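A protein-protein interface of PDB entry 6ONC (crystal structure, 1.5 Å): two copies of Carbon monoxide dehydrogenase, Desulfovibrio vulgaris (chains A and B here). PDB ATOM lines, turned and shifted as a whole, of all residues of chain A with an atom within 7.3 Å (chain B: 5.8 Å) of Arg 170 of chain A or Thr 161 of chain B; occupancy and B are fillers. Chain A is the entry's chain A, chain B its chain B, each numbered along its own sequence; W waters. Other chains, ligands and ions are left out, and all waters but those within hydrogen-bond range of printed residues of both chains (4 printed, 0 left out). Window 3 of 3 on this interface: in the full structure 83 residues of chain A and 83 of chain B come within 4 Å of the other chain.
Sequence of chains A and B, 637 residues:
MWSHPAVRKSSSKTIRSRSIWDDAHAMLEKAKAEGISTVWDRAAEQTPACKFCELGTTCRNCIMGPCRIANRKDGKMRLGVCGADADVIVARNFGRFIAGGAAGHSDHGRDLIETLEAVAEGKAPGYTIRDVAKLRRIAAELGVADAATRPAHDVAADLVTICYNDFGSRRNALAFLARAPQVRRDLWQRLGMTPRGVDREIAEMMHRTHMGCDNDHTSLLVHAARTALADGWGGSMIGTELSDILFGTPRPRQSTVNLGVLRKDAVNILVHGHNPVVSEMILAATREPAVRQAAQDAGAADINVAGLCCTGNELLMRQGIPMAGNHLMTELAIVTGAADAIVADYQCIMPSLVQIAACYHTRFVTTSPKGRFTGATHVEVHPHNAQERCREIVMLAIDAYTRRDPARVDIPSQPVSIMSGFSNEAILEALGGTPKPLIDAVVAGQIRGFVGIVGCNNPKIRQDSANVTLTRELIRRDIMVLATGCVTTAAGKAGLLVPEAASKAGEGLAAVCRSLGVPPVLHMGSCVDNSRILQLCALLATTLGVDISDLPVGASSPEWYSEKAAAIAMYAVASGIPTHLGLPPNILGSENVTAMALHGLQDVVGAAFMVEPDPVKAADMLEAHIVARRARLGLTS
The side-chain carboxylate (OE2) of Glu 117 of chain B lies within salt-bridge range of the guanidinium group (NH2) of Arg 170 of chain A (2.9 Å). NH1 of Arg 170 of chain A is in hydrogen-bond range of OG1 of Thr 161 of chain B (2.9 Å).
The side-chain amide nitrogen (ND2) of Asn 165 of chain B sits close to the backbone carbonyl oxygen (O) of Thr 161 of chain B (3.3 Å). O of Ala 157 of chain B sits at hydrogen-bond distance from OG1 of Thr 161 of chain B, 3.3 Å away.
Tyr 164 of chain B touches Ser 169 of chain A. Val 160 of chain B touches Arg 170 of chain A (CG1 to NH2, 3.8 Å). Arg 170 of chain A touches Tyr 164 of chain B (NE to CD2, 3.3 Å).
Printed residues of chain B within 4 Å of Ser 169 of chain A: Tyr 164. Of chain B, only Glu 117 (2.9 Å), Val 160 (3.8 Å), Thr 161 (2.9 Å) and Tyr 164 (3.3 Å) come within 4 Å of Arg 170 of chain A. Printed residues of chain A within 4 Å of Glu 117 of chain B: Arg 170 (2.9 Å). Of the printed residues of chain A, Val 160 of chain B touches Arg 170 (3.8 Å). Thr 161 of chain B touches just one residue of chain A: Arg 170 (2.9 Å). Of the printed residues of chain A, Tyr 164 of chain B touches Ser 169 and Arg 170.
Among the printed residues, Asp or Glu carboxylates within 4 Å of a Lys or Arg side-chain nitrogen of the other chain: Arg 170 of chain A with Glu 117 of chain B (2.9 Å).
Position printed for both chains: 165. Of the 5 pairs that touch across the chains among the printed residues, none has its exchanged pair printed and touching as well.
Water W1 lies within hydrogen-bond range of OE2 of Glu 117 of chain B (2.7 Å) and NE of Arg 170 of chain A (2.9 Å). Water W4 bridges the side-chain amide oxygen of Asn 165 of chain B (2.7 Å) and the guanidinium group of Arg 170 of chain A (2.9 Å). Water W2 lies within hydrogen-bond range of the backbone carbonyl oxygen of Tyr 164 of chain B and the backbone NH of Ser 169 of chain A. Water W3 lies within hydrogen-bond range of the backbone carbonyl oxygen of Ala 157 of chain B, the guanidinium group of Arg 170 of chain A and the side-chain hydroxyl of Thr 161 of chain B.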
ATOM      1  N   ASN A 165       3.240  16.927  20.383  1.00  0.00           N
ATOM      2  CA  ASN A 165       2.117  16.086  20.805  1.00  0.00           C
ATOM      3  C   ASN A 165       2.593  14.795  21.467  1.00  0.00           C
ATOM      4  O   ASN A 165       1.910  14.259  22.341  1.00  0.00           O
ATOM      5  CB  ASN A 165       1.165  15.805  19.632  1.00  0.00           C
ATOM      6  CG  ASN A 165       0.352  17.035  19.217  1.00  0.00           C
ATOM      7  OD1 ASN A 165       0.185  17.979  19.984  1.00  0.00           O
ATOM      8  ND2 ASN A 165      -0.161  17.016  17.991  1.00  0.00           N
ATOM      9  N   PHE A 167       5.048  14.768  23.460  1.00  0.00           N
ATOM     10  CA  PHE A 167       5.314  15.259  24.807  1.00  0.00           C
ATOM     11  C   PHE A 167       4.044  15.736  25.509  1.00  0.00           C
ATOM     12  O   PHE A 167       4.128  16.455  26.513  1.00  0.00           O
ATOM     13  CB  PHE A 167       6.373  16.370  24.769  1.00  0.00           C
ATOM     14  CG  PHE A 167       7.780  15.871  24.540  1.00  0.00           C
ATOM     15  CD1 PHE A 167       8.194  15.442  23.281  1.00  0.00           C
ATOM     16  CD2 PHE A 167       8.683  15.823  25.595  1.00  0.00           C
ATOM     17  CE1 PHE A 167       9.500  14.982  23.080  1.00  0.00           C
ATOM     18  CE2 PHE A 167       9.988  15.378  25.415  1.00  0.00           C
ATOM     19  CZ  PHE A 167      10.398  14.945  24.150  1.00  0.00           C
ATOM     20  N   GLY A 168       2.873  15.373  24.984  1.00  0.00           N
ATOM     21  CA  GLY A 168       1.613  15.626  25.636  1.00  0.00           C
ATOM     22  C   GLY A 168       0.981  14.338  26.122  1.00  0.00           C
ATOM     23  O   GLY A 168       1.598  13.271  26.121  1.00  0.00           O
ATOM     24  N   SER A 169      -0.284  14.450  26.529  1.00  0.00           N
ATOM     25  CA  SER A 169      -0.964  13.381  27.248  1.00  0.00           C
ATOM     26  C   SER A 169      -2.198  12.854  26.516  1.00  0.00           C
ATOM     27  O   SER A 169      -3.071  12.254  27.151  1.00  0.00           O
ATOM     28  CB  SER A 169      -1.318  13.850  28.669  1.00  0.00           C
ATOM     29  OG  SER A 169      -1.800  12.785  29.470  1.00  0.00           O
ATOM     30  N   ARG A 170      -2.269  13.018  25.189  1.00  0.00           N
ATOM     31  CA  ARG A 170      -3.462  12.639  24.438  1.00  0.00           C
ATOM     32  C   ARG A 170      -3.246  11.515  23.428  1.00  0.00           C
ATOM     33  O   ARG A 170      -4.214  11.107  22.771  1.00  0.00           O
ATOM     34  CB  ARG A 170      -4.091  13.862  23.745  1.00  0.00           C
ATOM     35  CG  ARG A 170      -4.458  14.996  24.714  1.00  0.00           C
ATOM     36  CD  ARG A 170      -5.320  16.048  24.049  1.00  0.00           C
ATOM     37  NE  ARG A 170      -6.726  15.653  24.028  1.00  0.00           N
ATOM     38  CZ  ARG A 170      -7.749  16.487  23.837  1.00  0.00           C
ATOM     39  NH1 ARG A 170      -7.539  17.782  23.634  1.00  0.00           N
ATOM     40  NH2 ARG A 170      -8.990  16.013  23.859  1.00  0.00           N
ATOM     41  N   ARG A 171      -2.024  11.005  23.282  1.00  0.00           N
ATOM     42  CA  ARG A 171      -1.745   9.954  22.310  1.00  0.00           C
ATOM     43  C   ARG A 171      -2.024   8.580  22.910  1.00  0.00           C
ATOM     44  O   ARG A 171      -1.940   8.377  24.125  1.00  0.00           O
ATOM     45  CB  ARG A 171      -0.280   9.991  21.859  1.00  0.00           C
ATOM     46  CG  ARG A 171       0.231  11.332  21.343  1.00  0.00           C
ATOM     47  CD  ARG A 171       0.144  11.443  19.825  1.00  0.00           C
ATOM     48  NE  ARG A 171       0.773  10.320  19.132  1.00  0.00           N
ATOM     49  CZ  ARG A 171       0.459   9.951  17.896  1.00  0.00           C
ATOM     50  NH1 ARG A 171      -0.477  10.612  17.229  1.00  0.00           N
ATOM     51  NH2 ARG A 171       1.061   8.916  17.328  1.00  0.00           N
ATOM     52  N   ASN A 172      -2.352   7.626  22.038  1.00  0.00           N
ATOM     53  CA  ASN A 172      -2.370   6.227  22.432  1.00  0.00           C
ATOM     54  C   ASN A 172      -1.034   5.553  22.157  1.00  0.00           C
ATOM     55  O   ASN A 172      -0.708   4.545  22.800  1.00  0.00           O
ATOM     56  CB  ASN A 172      -3.488   5.483  21.698  1.00  0.00           C
ATOM     57  CG  ASN A 172      -4.862   5.947  22.129  1.00  0.00           C
ATOM     58  OD1 ASN A 172      -5.099   6.200  23.312  1.00  0.00           O
ATOM     59  ND2 ASN A 172      -5.772   6.083  21.171  1.00  0.00           N
ATOM     60  N   ALA A 173      -0.253   6.105  21.232  1.00  0.00           N
ATOM     61  CA  ALA A 173       1.061   5.580  20.892  1.00  0.00           C
ATOM     62  C   ALA A 173       1.888   6.718  20.312  1.00  0.00           C
ATOM     63  O   ALA A 173       1.373   7.546  19.553  1.00  0.00           O
ATOM     64  CB  ALA A 173       0.954   4.448  19.861  1.00  0.00           C
ATOM     65  N   ARG A 196       3.161   6.066  25.296  1.00  0.00           N
ATOM     66  CA  ARG A 196       2.100   6.993  24.900  1.00  0.00           C
ATOM     67  C   ARG A 196       2.548   8.442  24.879  1.00  0.00           C
ATOM     68  O   ARG A 196       2.121   9.204  24.010  1.00  0.00           O
ATOM     69  CB  ARG A 196       0.926   6.885  25.875  1.00  0.00           C
ATOM     70  CG  ARG A 196       0.386   5.480  26.048  1.00  0.00           C
ATOM     71  CD  ARG A 196      -0.408   5.388  27.332  1.00  0.00           C
ATOM     72  NE  ARG A 196       0.472   5.439  28.495  1.00  0.00           N
ATOM     73  CZ  ARG A 196       0.045   5.367  29.754  1.00  0.00           C
ATOM     74  NH1 ARG A 196      -1.255   5.232  30.009  1.00  0.00           N
ATOM     75  NH2 ARG A 196       0.916   5.403  30.753  1.00  0.00           N
ATOM     76  N   GLY A 197       3.360   8.836  25.847  1.00  0.00           N
ATOM     77  CA  GLY A 197       3.826  10.204  25.969  1.00  0.00           C
ATOM     78  C   GLY A 197       5.196  10.199  26.602  1.00  0.00           C
ATOM     79  O   GLY A 197       5.426   9.477  27.573  1.00  0.00           O
ATOM     80  N   ARG A 200       4.846  11.721  29.940  1.00  0.00           N
ATOM     81  CA  ARG A 200       3.813  11.047  30.717  1.00  0.00           C
ATOM     82  C   ARG A 200       4.340   9.779  31.374  1.00  0.00           C
ATOM     83  O   ARG A 200       4.038   9.516  32.543  1.00  0.00           O
ATOM     84  CB  ARG A 200       2.599  10.728  29.852  1.00  0.00           C
ATOM     85  CG  ARG A 200       1.600   9.862  30.604  1.00  0.00           C
ATOM     86  CD  ARG A 200       0.337   9.609  29.831  1.00  0.00           C
ATOM     87  NE  ARG A 200      -0.638   8.955  30.691  1.00  0.00           N
ATOM     88  CZ  ARG A 200      -1.859   8.601  30.305  1.00  0.00           C
ATOM     89  NH1 ARG A 200      -2.251   8.827  29.055  1.00  0.00           N
ATOM     90  NH2 ARG A 200      -2.685   8.028  31.174  1.00  0.00           N
ATOM     91  N   GLU B 117     -13.401  14.116  29.689  1.00  0.00           N
ATOM     92  CA  GLU B 117     -13.406  13.867  28.256  1.00  0.00           C
ATOM     93  C   GLU B 117     -14.354  12.730  27.899  1.00  0.00           C
ATOM     94  O   GLU B 117     -15.132  12.840  26.943  1.00  0.00           O
ATOM     95  CB  GLU B 117     -11.991  13.538  27.789  1.00  0.00           C
ATOM     96  CG  GLU B 117     -11.891  13.275  26.301  1.00  0.00           C
ATOM     97  CD  GLU B 117     -10.486  12.932  25.871  1.00  0.00           C
ATOM     98  OE1 GLU B 117      -9.815  12.136  26.567  1.00  0.00           O
ATOM     99  OE2 GLU B 117     -10.052  13.472  24.838  1.00  0.00           O
ATOM    100  N   ALA B 156     -17.308  21.392  27.734  1.00  0.00           N
ATOM    101  CA  ALA B 156     -16.454  20.432  28.433  1.00  0.00           C
ATOM    102  C   ALA B 156     -15.299  19.981  27.549  1.00  0.00           C
ATOM    103  O   ALA B 156     -14.156  19.888  28.010  1.00  0.00           O
ATOM    104  CB  ALA B 156     -17.277  19.226  28.897  1.00  0.00           C
ATOM    105  N   ALA B 157     -15.573  19.696  26.272  1.00  0.00           N
ATOM    106  CA  ALA B 157     -14.494  19.284  25.375  1.00  0.00           C
ATOM    107  C   ALA B 157     -13.427  20.363  25.267  1.00  0.00           C
ATOM    108  O   ALA B 157     -12.227  20.059  25.228  1.00  0.00           O
ATOM    109  CB  ALA B 157     -15.047  18.968  23.985  1.00  0.00           C
ATOM    110  N   ASP B 158     -13.839  21.630  25.201  1.00  0.00           N
ATOM    111  CA  ASP B 158     -12.855  22.705  25.115  1.00  0.00           C
ATOM    112  C   ASP B 158     -12.069  22.865  26.414  1.00  0.00           C
ATOM    113  O   ASP B 158     -10.878  23.199  26.374  1.00  0.00           O
ATOM    114  CB  ASP B 158     -13.520  24.020  24.710  1.00  0.00           C
ATOM    115  CG  ASP B 158     -13.902  24.051  23.244  1.00  0.00           C
ATOM    116  OD1 ASP B 158     -13.510  23.122  22.499  1.00  0.00           O
ATOM    117  OD2 ASP B 158     -14.588  25.008  22.833  1.00  0.00           O
ATOM    118  N   LEU B 159     -12.714  22.647  27.562  1.00  0.00           N
ATOM    119  CA  LEU B 159     -11.993  22.699  28.830  1.00  0.00           C
ATOM    120  C   LEU B 159     -11.009  21.543  28.940  1.00  0.00           C
ATOM    121  O   LEU B 159      -9.890  21.718  29.443  1.00  0.00           O
ATOM    122  CB  LEU B 159     -12.979  22.709  30.003  1.00  0.00           C
ATOM    123  CG  LEU B 159     -12.362  22.675  31.406  1.00  0.00           C
ATOM    124  CD1 LEU B 159     -11.450  23.881  31.609  1.00  0.00           C
ATOM    125  CD2 LEU B 159     -13.465  22.670  32.444  1.00  0.00           C
ATOM    126  N   VAL B 160     -11.413  20.359  28.472  1.00  0.00           N
ATOM    127  CA  VAL B 160     -10.515  19.204  28.428  1.00  0.00           C
ATOM    128  C   VAL B 160      -9.255  19.533  27.633  1.00  0.00           C
ATOM    129  O   VAL B 160      -8.133  19.244  28.064  1.00  0.00           O
ATOM    130  CB  VAL B 160     -11.258  17.981  27.858  1.00  0.00           C
ATOM    131  CG1 VAL B 160     -10.282  16.922  27.326  1.00  0.00           C
ATOM    132  CG2 VAL B 160     -12.178  17.392  28.919  1.00  0.00           C
ATOM    133  N   THR B 161      -9.419  20.159  26.466  1.00  0.00           N
ATOM    134  CA  THR B 161      -8.260  20.557  25.674  1.00  0.00           C
ATOM    135  C   THR B 161      -7.338  21.517  26.429  1.00  0.00           C
ATOM    136  O   THR B 161      -6.112  21.356  26.385  1.00  0.00           O
ATOM    137  CB  THR B 161      -8.715  21.134  24.336  1.00  0.00           C
ATOM    138  OG1 THR B 161      -9.360  20.093  23.591  1.00  0.00           O
ATOM    139  CG2 THR B 161      -7.523  21.667  23.531  1.00  0.00           C
ATOM    140  N   ILE B 162      -7.902  22.512  27.122  1.00  0.00           N
ATOM    141  CA  ILE B 162      -7.070  23.439  27.894  1.00  0.00           C
ATOM    142  C   ILE B 162      -6.303  22.686  28.973  1.00  0.00           C
ATOM    143  O   ILE B 162      -5.089  22.863  29.137  1.00  0.00           O
ATOM    144  CB  ILE B 162      -7.930  24.560  28.506  1.00  0.00           C
ATOM    145  CG1 ILE B 162      -8.446  25.485  27.401  1.00  0.00           C
ATOM    146  CG2 ILE B 162      -7.114  25.330  29.537  1.00  0.00           C
ATOM    147  CD1 ILE B 162      -9.453  26.512  27.884  1.00  0.00           C
ATOM    148  N   CYS B 163      -7.003  21.821  29.711  1.00  0.00           N
ATOM    149  CA  CYS B 163      -6.345  21.074  30.781  1.00  0.00           C
ATOM    150  C   CYS B 163      -5.254  20.153  30.233  1.00  0.00           C
ATOM    151  O   CYS B 163      -4.147  20.101  30.783  1.00  0.00           O
ATOM    152  CB  CYS B 163      -7.377  20.314  31.607  1.00  0.00           C
ATOM    153  SG  CYS B 163      -8.483  21.398  32.563  1.00  0.00           S
ATOM    154  N   TYR B 164      -5.544  19.410  29.153  1.00  0.00           N
ATOM    155  CA  TYR B 164      -4.511  18.560  28.559  1.00  0.00           C
ATOM    156  C   TYR B 164      -3.316  19.362  28.061  1.00  0.00           C
ATOM    157  O   TYR B 164      -2.178  18.882  28.124  1.00  0.00           O
ATOM    158  CB  TYR B 164      -5.094  17.716  27.428  1.00  0.00           C
ATOM    159  CG  TYR B 164      -5.601  16.352  27.843  1.00  0.00           C
ATOM    160  CD1 TYR B 164      -4.871  15.533  28.708  1.00  0.00           C
ATOM    161  CD2 TYR B 164      -6.804  15.866  27.352  1.00  0.00           C
ATOM    162  CE1 TYR B 164      -5.337  14.268  29.067  1.00  0.00           C
ATOM    163  CE2 TYR B 164      -7.273  14.611  27.703  1.00  0.00           C
ATOM    164  CZ  TYR B 164      -6.536  13.817  28.568  1.00  0.00           C
ATOM    165  OH  TYR B 164      -6.998  12.564  28.929  1.00  0.00           O
ATOM    166  N   ASN B 165      -3.539  20.579  27.570  1.00  0.00           N
ATOM    167  CA  ASN B 165      -2.409  21.390  27.127  1.00  0.00           C
ATOM    168  C   ASN B 165      -1.476  21.749  28.282  1.00  0.00           C
ATOM    169  O   ASN B 165      -0.272  21.925  28.076  1.00  0.00           O
ATOM    170  CB  ASN B 165      -2.892  22.625  26.366  1.00  0.00           C
ATOM    171  CG  ASN B 165      -3.483  22.284  24.998  1.00  0.00           C
ATOM    172  OD1 ASN B 165      -3.269  21.196  24.464  1.00  0.00           O
ATOM    173  ND2 ASN B 165      -4.234  23.221  24.428  1.00  0.00           N
ATOM    174  N   ASP B 166      -1.997  21.829  29.509  1.00  0.00           N
ATOM    175  CA  ASP B 166      -1.122  22.005  30.663  1.00  0.00           C
ATOM    176  C   ASP B 166      -0.303  20.762  30.966  1.00  0.00           C
ATOM    177  O   ASP B 166       0.707  20.864  31.671  1.00  0.00           O
ATOM    178  CB  ASP B 166      -1.927  22.448  31.893  1.00  0.00           C
ATOM    179  CG  ASP B 166      -2.141  23.969  31.927  1.00  0.00           C
ATOM    180  OD1 ASP B 166      -1.798  24.664  30.935  1.00  0.00           O
ATOM    181  OD2 ASP B 166      -2.641  24.458  32.950  1.00  0.00           O
HETATM  182  O   HOH W   1      -7.498  12.859  24.188  1.00  0.00           O
HETATM  183  O   HOH W   2      -1.588  16.925  26.283  1.00  0.00           O
HETATM  184  O   HOH W   3     -11.419  17.807  23.713  1.00  0.00           O
HETATM  185  O   HOH W   4      -5.076  19.311  23.666  1.00  0.00           O
